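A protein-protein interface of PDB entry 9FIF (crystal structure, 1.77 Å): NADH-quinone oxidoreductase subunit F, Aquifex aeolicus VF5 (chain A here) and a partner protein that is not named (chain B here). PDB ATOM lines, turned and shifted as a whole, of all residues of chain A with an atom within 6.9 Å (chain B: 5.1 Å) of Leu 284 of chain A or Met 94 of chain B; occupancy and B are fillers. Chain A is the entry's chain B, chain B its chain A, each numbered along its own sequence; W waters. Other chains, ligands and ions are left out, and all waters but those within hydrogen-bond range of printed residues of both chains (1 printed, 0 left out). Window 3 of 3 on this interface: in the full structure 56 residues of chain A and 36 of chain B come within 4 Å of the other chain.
Water W1 bridges O of Leu 93 of chain B and NZ of Lys 257 of chain A.
The backbone NH (N) of Val 324 of chain A lies within hydrogen-bond range of the backbone carbonyl oxygen (O) of Ser 255 of chain A, 3.0 Å away. O of Lys 257 of chain A sits at hydrogen-bond distance from N of Leu 284 of chain A. N of Lys 257 of chain A sits at hydrogen-bond distance from O of Val 324 of chain A (2.9 Å).
OG of Ser 255 of chain A touches CG1 of Val 90 of chain B (3.7 Å). Gly 256 of chain A touches Val 90 of chain B. Met 94 of chain B touches Gly 256 of chain A. Lys 257 of chain A touches Met 94 of chain B (CE to SD, 3.6 Å). Leu 284 of chain A touches Met 94 of chain B.
Of the 9 printed residues of chain B, 2 touch a printed residue of chain A. Printed residues of chain B that touch a printed residue of chain A: Val 90 and Met 94. Hydrophobic or aromatic side chains of chain B that line the printed part of chain A: Val 90 and Met 94. Among the printed residues, no Asp or Glu carboxylate lies within 4 Å of a Lys or Arg side-chain nitrogen of the other chain.
Printed residues of chain B within 4 Å of Ser 255 of chain A: Val 90 (3.7 Å). Lys 259 of chain A touches none of the printed residues of chain B. Leu 284 of chain A touches just one residue of chain B: Met 94 (3.9 Å). Of the printed residues of chain A, Val 90 of chain B touches Ser 255 and Gly 256. Of the printed residues of chain A, Met 94 of chain B touches Gly 256 (3.9 Å), Lys 257 (3.6 Å) and Leu 284 (3.9 Å). The nearest printed residue of chain B that does not touch Leu 284 of chain A is Leu 93 of chain B (7.8 Å). The nearest printed residue of chain B that does not touch Ser 255 of chain A is Met 94 of chain B (6.2 Å).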
ATOM      1  N   SER A 255     -22.634 -11.163 -11.607  1.00  0.00           N
ATOM      2  CA  SER A 255     -23.986 -10.705 -11.862  1.00  0.00           C
ATOM      3  C   SER A 255     -24.998 -11.469 -11.013  1.00  0.00           C
ATOM      4  O   SER A 255     -24.644 -12.326 -10.198  1.00  0.00           O
ATOM      5  CB  SER A 255     -24.285 -10.851 -13.335  1.00  0.00           C
ATOM      6  OG  SER A 255     -24.252 -12.220 -13.716  1.00  0.00           O
ATOM      7  N   GLY A 256     -26.282 -11.168 -11.248  1.00  0.00           N
ATOM      8  CA  GLY A 256     -27.362 -11.732 -10.464  1.00  0.00           C
ATOM      9  C   GLY A 256     -27.556 -10.980  -9.143  1.00  0.00           C
ATOM     10  O   GLY A 256     -27.444  -9.747  -9.077  1.00  0.00           O
ATOM     11  N   LYS A 257     -27.819 -11.747  -8.080  1.00  0.00           N
ATOM     12  CA  LYS A 257     -28.363 -11.220  -6.837  1.00  0.00           C
ATOM     13  C   LYS A 257     -27.276 -10.697  -5.892  1.00  0.00           C
ATOM     14  O   LYS A 257     -27.294 -10.999  -4.696  1.00  0.00           O
ATOM     15  CB  LYS A 257     -29.196 -12.337  -6.195  1.00  0.00           C
ATOM     16  CG  LYS A 257     -30.352 -12.810  -7.061  1.00  0.00           C
ATOM     17  CD  LYS A 257     -31.337 -11.686  -7.363  1.00  0.00           C
ATOM     18  CE  LYS A 257     -32.527 -12.114  -8.158  1.00  0.00           C
ATOM     19  NZ  LYS A 257     -33.390 -12.968  -7.351  1.00  0.00           N
ATOM     20  N   VAL A 258     -26.383  -9.845  -6.411  1.00  0.00           N
ATOM     21  CA  VAL A 258     -25.378  -9.181  -5.600  1.00  0.00           C
ATOM     22  C   VAL A 258     -25.666  -7.680  -5.630  1.00  0.00           C
ATOM     23  O   VAL A 258     -26.310  -7.183  -6.552  1.00  0.00           O
ATOM     24  CB  VAL A 258     -23.946  -9.474  -6.091  1.00  0.00           C
ATOM     25  CG1 VAL A 258     -23.607 -10.966  -6.009  1.00  0.00           C
ATOM     26  CG2 VAL A 258     -23.743  -8.953  -7.504  1.00  0.00           C
ATOM     27  N   LYS A 259     -25.149  -6.966  -4.634  1.00  0.00           N
ATOM     28  CA  LYS A 259     -25.402  -5.543  -4.502  1.00  0.00           C
ATOM     29  C   LYS A 259     -24.599  -4.734  -5.512  1.00  0.00           C
ATOM     30  O   LYS A 259     -25.081  -3.694  -5.941  1.00  0.00           O
ATOM     31  CB  LYS A 259     -25.069  -5.053  -3.091  1.00  0.00           C
ATOM     32  CG  LYS A 259     -25.922  -5.663  -2.002  1.00  0.00           C
ATOM     33  CD  LYS A 259     -25.790  -4.877  -0.706  1.00  0.00           C
ATOM     34  CE  LYS A 259     -26.537  -5.430   0.447  1.00  0.00           C
ATOM     35  NZ  LYS A 259     -25.956  -6.711   0.844  1.00  0.00           N
ATOM     36  N   LYS A 260     -23.380  -5.188  -5.844  1.00  0.00           N
ATOM     37  CA  LYS A 260     -22.504  -4.477  -6.772  1.00  0.00           C
ATOM     38  C   LYS A 260     -22.144  -5.361  -7.971  1.00  0.00           C
ATOM     39  O   LYS A 260     -20.993  -5.750  -8.146  1.00  0.00           O
ATOM     40  CB  LYS A 260     -21.217  -4.009  -6.067  1.00  0.00           C
ATOM     41  CG  LYS A 260     -21.384  -3.035  -4.890  1.00  0.00           C
ATOM     42  CD  LYS A 260     -20.123  -2.854  -4.050  1.00  0.00           C
ATOM     43  CE  LYS A 260     -18.856  -2.680  -4.881  1.00  0.00           C
ATOM     44  NZ  LYS A 260     -17.668  -2.683  -4.012  1.00  0.00           N
ATOM     45  N   PRO A 261     -23.081  -5.657  -8.894  1.00  0.00           N
ATOM     46  CA  PRO A 261     -22.730  -6.422 -10.089  1.00  0.00           C
ATOM     47  C   PRO A 261     -21.773  -5.610 -10.959  1.00  0.00           C
ATOM     48  O   PRO A 261     -21.878  -4.387 -11.024  1.00  0.00           O
ATOM     49  CB  PRO A 261     -24.086  -6.670 -10.749  1.00  0.00           C
ATOM     50  CG  PRO A 261     -24.909  -5.493 -10.331  1.00  0.00           C
ATOM     51  CD  PRO A 261     -24.480  -5.203  -8.894  1.00  0.00           C
ATOM     52  N   GLY A 281     -20.248  -6.760  -2.526  1.00  0.00           N
ATOM     53  CA  GLY A 281     -21.138  -6.081  -1.584  1.00  0.00           C
ATOM     54  C   GLY A 281     -22.165  -6.999  -0.921  1.00  0.00           C
ATOM     55  O   GLY A 281     -23.035  -6.539  -0.168  1.00  0.00           O
ATOM     56  N   GLY A 282     -22.049  -8.310  -1.169  1.00  0.00           N
ATOM     57  CA  GLY A 282     -22.977  -9.270  -0.597  1.00  0.00           C
ATOM     58  C   GLY A 282     -24.207  -9.399  -1.483  1.00  0.00           C
ATOM     59  O   GLY A 282     -24.211  -8.933  -2.616  1.00  0.00           O
ATOM     60  N   THR A 283     -25.246 -10.038  -0.944  1.00  0.00           N
ATOM     61  CA  THR A 283     -26.422 -10.372  -1.722  1.00  0.00           C
ATOM     62  C   THR A 283     -27.457  -9.261  -1.600  1.00  0.00           C
ATOM     63  O   THR A 283     -27.503  -8.536  -0.612  1.00  0.00           O
ATOM     64  CB  THR A 283     -26.998 -11.716  -1.273  1.00  0.00           C
ATOM     65  OG1 THR A 283     -27.330 -11.631   0.118  1.00  0.00           O
ATOM     66  CG2 THR A 283     -26.031 -12.861  -1.504  1.00  0.00           C
ATOM     67  N   LEU A 284     -28.313  -9.181  -2.622  1.00  0.00           N
ATOM     68  CA  LEU A 284     -29.490  -8.336  -2.568  1.00  0.00           C
ATOM     69  C   LEU A 284     -30.362  -8.797  -1.409  1.00  0.00           C
ATOM     70  O   LEU A 284     -30.658  -9.991  -1.294  1.00  0.00           O
ATOM     71  CB  LEU A 284     -30.272  -8.406  -3.877  1.00  0.00           C
ATOM     72  CG  LEU A 284     -29.631  -7.723  -5.085  1.00  0.00           C
ATOM     73  CD1 LEU A 284     -30.548  -7.938  -6.278  1.00  0.00           C
ATOM     74  CD2 LEU A 284     -29.384  -6.238  -4.851  1.00  0.00           C
ATOM     75  N   GLY A 285     -30.734  -7.832  -0.564  1.00  0.00           N
ATOM     76  CA  GLY A 285     -31.599  -8.059   0.588  1.00  0.00           C
ATOM     77  C   GLY A 285     -30.917  -8.902   1.665  1.00  0.00           C
ATOM     78  O   GLY A 285     -31.587  -9.421   2.545  1.00  0.00           O
ATOM     79  N   ASN A 286     -29.592  -9.083   1.565  1.00  0.00           N
ATOM     80  CA  ASN A 286     -28.855  -9.949   2.475  1.00  0.00           C
ATOM     81  C   ASN A 286     -29.498 -11.331   2.552  1.00  0.00           C
ATOM     82  O   ASN A 286     -29.453 -11.978   3.591  1.00  0.00           O
ATOM     83  CB  ASN A 286     -28.706  -9.305   3.849  1.00  0.00           C
ATOM     84  CG  ASN A 286     -27.933  -8.014   3.758  1.00  0.00           C
ATOM     85  OD1 ASN A 286     -28.394  -6.971   4.221  1.00  0.00           O
ATOM     86  ND2 ASN A 286     -26.745  -8.058   3.181  1.00  0.00           N
ATOM     87  N   LYS A 287     -30.072 -11.795   1.445  1.00  0.00           N
ATOM     88  CA  LYS A 287     -30.622 -13.138   1.392  1.00  0.00           C
ATOM     89  C   LYS A 287     -29.485 -14.151   1.250  1.00  0.00           C
ATOM     90  O   LYS A 287     -28.388 -13.815   0.785  1.00  0.00           O
ATOM     91  CB  LYS A 287     -31.604 -13.213   0.221  1.00  0.00           C
ATOM     92  CG  LYS A 287     -32.883 -12.402   0.365  1.00  0.00           C
ATOM     93  CD  LYS A 287     -33.530 -12.169  -0.998  1.00  0.00           C
ATOM     94  CE  LYS A 287     -35.028 -12.070  -0.996  1.00  0.00           C
ATOM     95  NZ  LYS A 287     -35.522 -12.448  -2.331  1.00  0.00           N
ATOM     96  N   LYS A 288     -29.769 -15.396   1.638  1.00  0.00           N
ATOM     97  CA  LYS A 288     -28.770 -16.447   1.611  1.00  0.00           C
ATOM     98  C   LYS A 288     -28.479 -16.851   0.168  1.00  0.00           C
ATOM     99  O   LYS A 288     -29.385 -16.937  -0.664  1.00  0.00           O
ATOM    100  CB  LYS A 288     -29.236 -17.660   2.426  1.00  0.00           C
ATOM    101  CG  LYS A 288     -29.188 -17.449   3.927  1.00  0.00           C
ATOM    102  CD  LYS A 288     -29.590 -18.694   4.706  1.00  0.00           C
ATOM    103  CE  LYS A 288     -29.570 -18.471   6.182  1.00  0.00           C
ATOM    104  NZ  LYS A 288     -29.973 -19.722   6.831  1.00  0.00           N
ATOM    105  N   VAL A 324     -24.985 -15.116  -9.270  1.00  0.00           N
ATOM    106  CA  VAL A 324     -25.429 -15.442  -7.922  1.00  0.00           C
ATOM    107  C   VAL A 324     -26.952 -15.579  -7.885  1.00  0.00           C
ATOM    108  O   VAL A 324     -27.669 -14.674  -8.321  1.00  0.00           O
ATOM    109  CB  VAL A 324     -24.924 -14.387  -6.913  1.00  0.00           C
ATOM    110  CG1 VAL A 324     -25.442 -14.659  -5.511  1.00  0.00           C
ATOM    111  CG2 VAL A 324     -23.397 -14.305  -6.914  1.00  0.00           C
ATOM    112  N   THR A 326     -30.091 -16.530  -5.063  1.00  0.00           N
ATOM    113  CA  THR A 326     -30.350 -16.546  -3.632  1.00  0.00           C
ATOM    114  C   THR A 326     -31.545 -17.443  -3.322  1.00  0.00           C
ATOM    115  O   THR A 326     -32.118 -18.074  -4.208  1.00  0.00           O
ATOM    116  CB  THR A 326     -30.522 -15.126  -3.079  1.00  0.00           C
ATOM    117  OG1 THR A 326     -31.511 -14.500  -3.885  1.00  0.00           O
ATOM    118  CG2 THR A 326     -29.233 -14.325  -3.154  1.00  0.00           C
ATOM    119  N   VAL B  90     -29.576 -14.494 -16.684  1.00  0.00           N
ATOM    120  CA  VAL B  90     -29.393 -13.401 -15.730  1.00  0.00           C
ATOM    121  C   VAL B  90     -30.499 -12.364 -15.929  1.00  0.00           C
ATOM    122  O   VAL B  90     -31.148 -11.955 -14.961  1.00  0.00           O
ATOM    123  CB  VAL B  90     -27.988 -12.771 -15.731  1.00  0.00           C
ATOM    124  CG1 VAL B  90     -27.807 -11.821 -14.551  1.00  0.00           C
ATOM    125  CG2 VAL B  90     -26.911 -13.842 -15.697  1.00  0.00           C
ATOM    126  N   CYS B  91     -30.793 -12.005 -17.184  1.00  0.00           N
ATOM    127  CA  CYS B  91     -31.859 -11.047 -17.426  1.00  0.00           C
ATOM    128  C   CYS B  91     -33.203 -11.586 -16.942  1.00  0.00           C
ATOM    129  O   CYS B  91     -34.022 -10.817 -16.419  1.00  0.00           O
ATOM    130  CB  CYS B  91     -31.846 -10.562 -18.870  1.00  0.00           C
ATOM    131  SG  CYS B  91     -30.346  -9.608 -19.221  1.00  0.00           S
ATOM    132  N   HIS B  92     -33.417 -12.899 -17.091  1.00  0.00           N
ATOM    133  CA  HIS B  92     -34.656 -13.513 -16.660  1.00  0.00           C
ATOM    134  C   HIS B  92     -34.817 -13.343 -15.151  1.00  0.00           C
ATOM    135  O   HIS B  92     -35.887 -12.939 -14.681  1.00  0.00           O
ATOM    136  CB  HIS B  92     -34.726 -14.982 -17.090  1.00  0.00           C
ATOM    137  CG  HIS B  92     -35.983 -15.599 -16.559  1.00  0.00           C
ATOM    138  ND1 HIS B  92     -37.224 -15.334 -17.100  1.00  0.00           N
ATOM    139  CD2 HIS B  92     -36.186 -16.386 -15.505  1.00  0.00           C
ATOM    140  CE1 HIS B  92     -38.150 -15.971 -16.392  1.00  0.00           C
ATOM    141  NE2 HIS B  92     -37.543 -16.621 -15.415  1.00  0.00           N
ATOM    142  N   LEU B  93     -33.745 -13.664 -14.420  1.00  0.00           N
ATOM    143  CA  LEU B  93     -33.683 -13.498 -12.971  1.00  0.00           C
ATOM    144  C   LEU B  93     -34.028 -12.077 -12.545  1.00  0.00           C
ATOM    145  O   LEU B  93     -34.682 -11.897 -11.521  1.00  0.00           O
ATOM    146  CB  LEU B  93     -32.288 -13.813 -12.429  1.00  0.00           C
ATOM    147  CG  LEU B  93     -31.943 -15.282 -12.198  1.00  0.00           C
ATOM    148  CD1 LEU B  93     -30.524 -15.322 -11.676  1.00  0.00           C
ATOM    149  CD2 LEU B  93     -32.893 -15.959 -11.233  1.00  0.00           C
ATOM    150  N   MET B  94     -33.494 -11.085 -13.268  1.00  0.00           N
ATOM    151  CA  MET B  94     -33.512  -9.706 -12.818  1.00  0.00           C
ATOM    152  C   MET B  94     -34.636  -8.898 -13.469  1.00  0.00           C
ATOM    153  O   MET B  94     -34.805  -7.730 -13.115  1.00  0.00           O
ATOM    154  CB  MET B  94     -32.162  -9.037 -13.105  1.00  0.00           C
ATOM    155  CG  MET B  94     -30.973  -9.791 -12.545  1.00  0.00           C
ATOM    156  SD  MET B  94     -31.055 -10.069 -10.766  1.00  0.00           S
ATOM    157  CE  MET B  94     -30.972  -8.372 -10.170  1.00  0.00           C
ATOM    158  N   GLY B  95     -35.401  -9.491 -14.399  1.00  0.00           N
ATOM    159  CA  GLY B  95     -36.693  -8.926 -14.774  1.00  0.00           C
ATOM    160  C   GLY B  95     -36.952  -8.753 -16.279  1.00  0.00           C
ATOM    161  O   GLY B  95     -37.647  -7.806 -16.663  1.00  0.00           O
ATOM    162  N   THR B  96     -36.488  -9.683 -17.131  1.00  0.00           N
ATOM    163  CA  THR B  96     -36.904  -9.695 -18.534  1.00  0.00           C
ATOM    164  C   THR B  96     -38.417  -9.498 -18.658  1.00  0.00           C
ATOM    165  O   THR B  96     -38.874  -8.773 -19.543  1.00  0.00           O
ATOM    166  CB  THR B  96     -36.484 -10.979 -19.249  1.00  0.00           C
ATOM    167  OG1 THR B  96     -35.063 -11.020 -19.234  1.00  0.00           O
ATOM    168  CG2 THR B  96     -36.961 -11.029 -20.692  1.00  0.00           C
ATOM    169  N   ALA B 134     -28.494  -6.270 -16.137  1.00  0.00           N
ATOM    170  CA  ALA B 134     -29.757  -6.946 -16.392  1.00  0.00           C
ATOM    171  C   ALA B 134     -30.923  -6.152 -15.819  1.00  0.00           C
ATOM    172  O   ALA B 134     -30.792  -5.566 -14.743  1.00  0.00           O
ATOM    173  CB  ALA B 134     -29.731  -8.336 -15.786  1.00  0.00           C
ATOM    174  N   PRO B 135     -32.109  -6.126 -16.470  1.00  0.00           N
ATOM    175  CA  PRO B 135     -32.339  -6.736 -17.785  1.00  0.00           C
ATOM    176  C   PRO B 135     -31.940  -5.808 -18.928  1.00  0.00           C
ATOM    177  O   PRO B 135     -32.201  -4.605 -18.873  1.00  0.00           O
ATOM    178  CB  PRO B 135     -33.841  -7.045 -17.808  1.00  0.00           C
ATOM    179  CG  PRO B 135     -34.440  -6.194 -16.719  1.00  0.00           C
ATOM    180  CD  PRO B 135     -33.341  -5.578 -15.899  1.00  0.00           C
HETATM  181  O   HOH W   1     -35.742 -13.221  -9.485  1.00  0.00           O
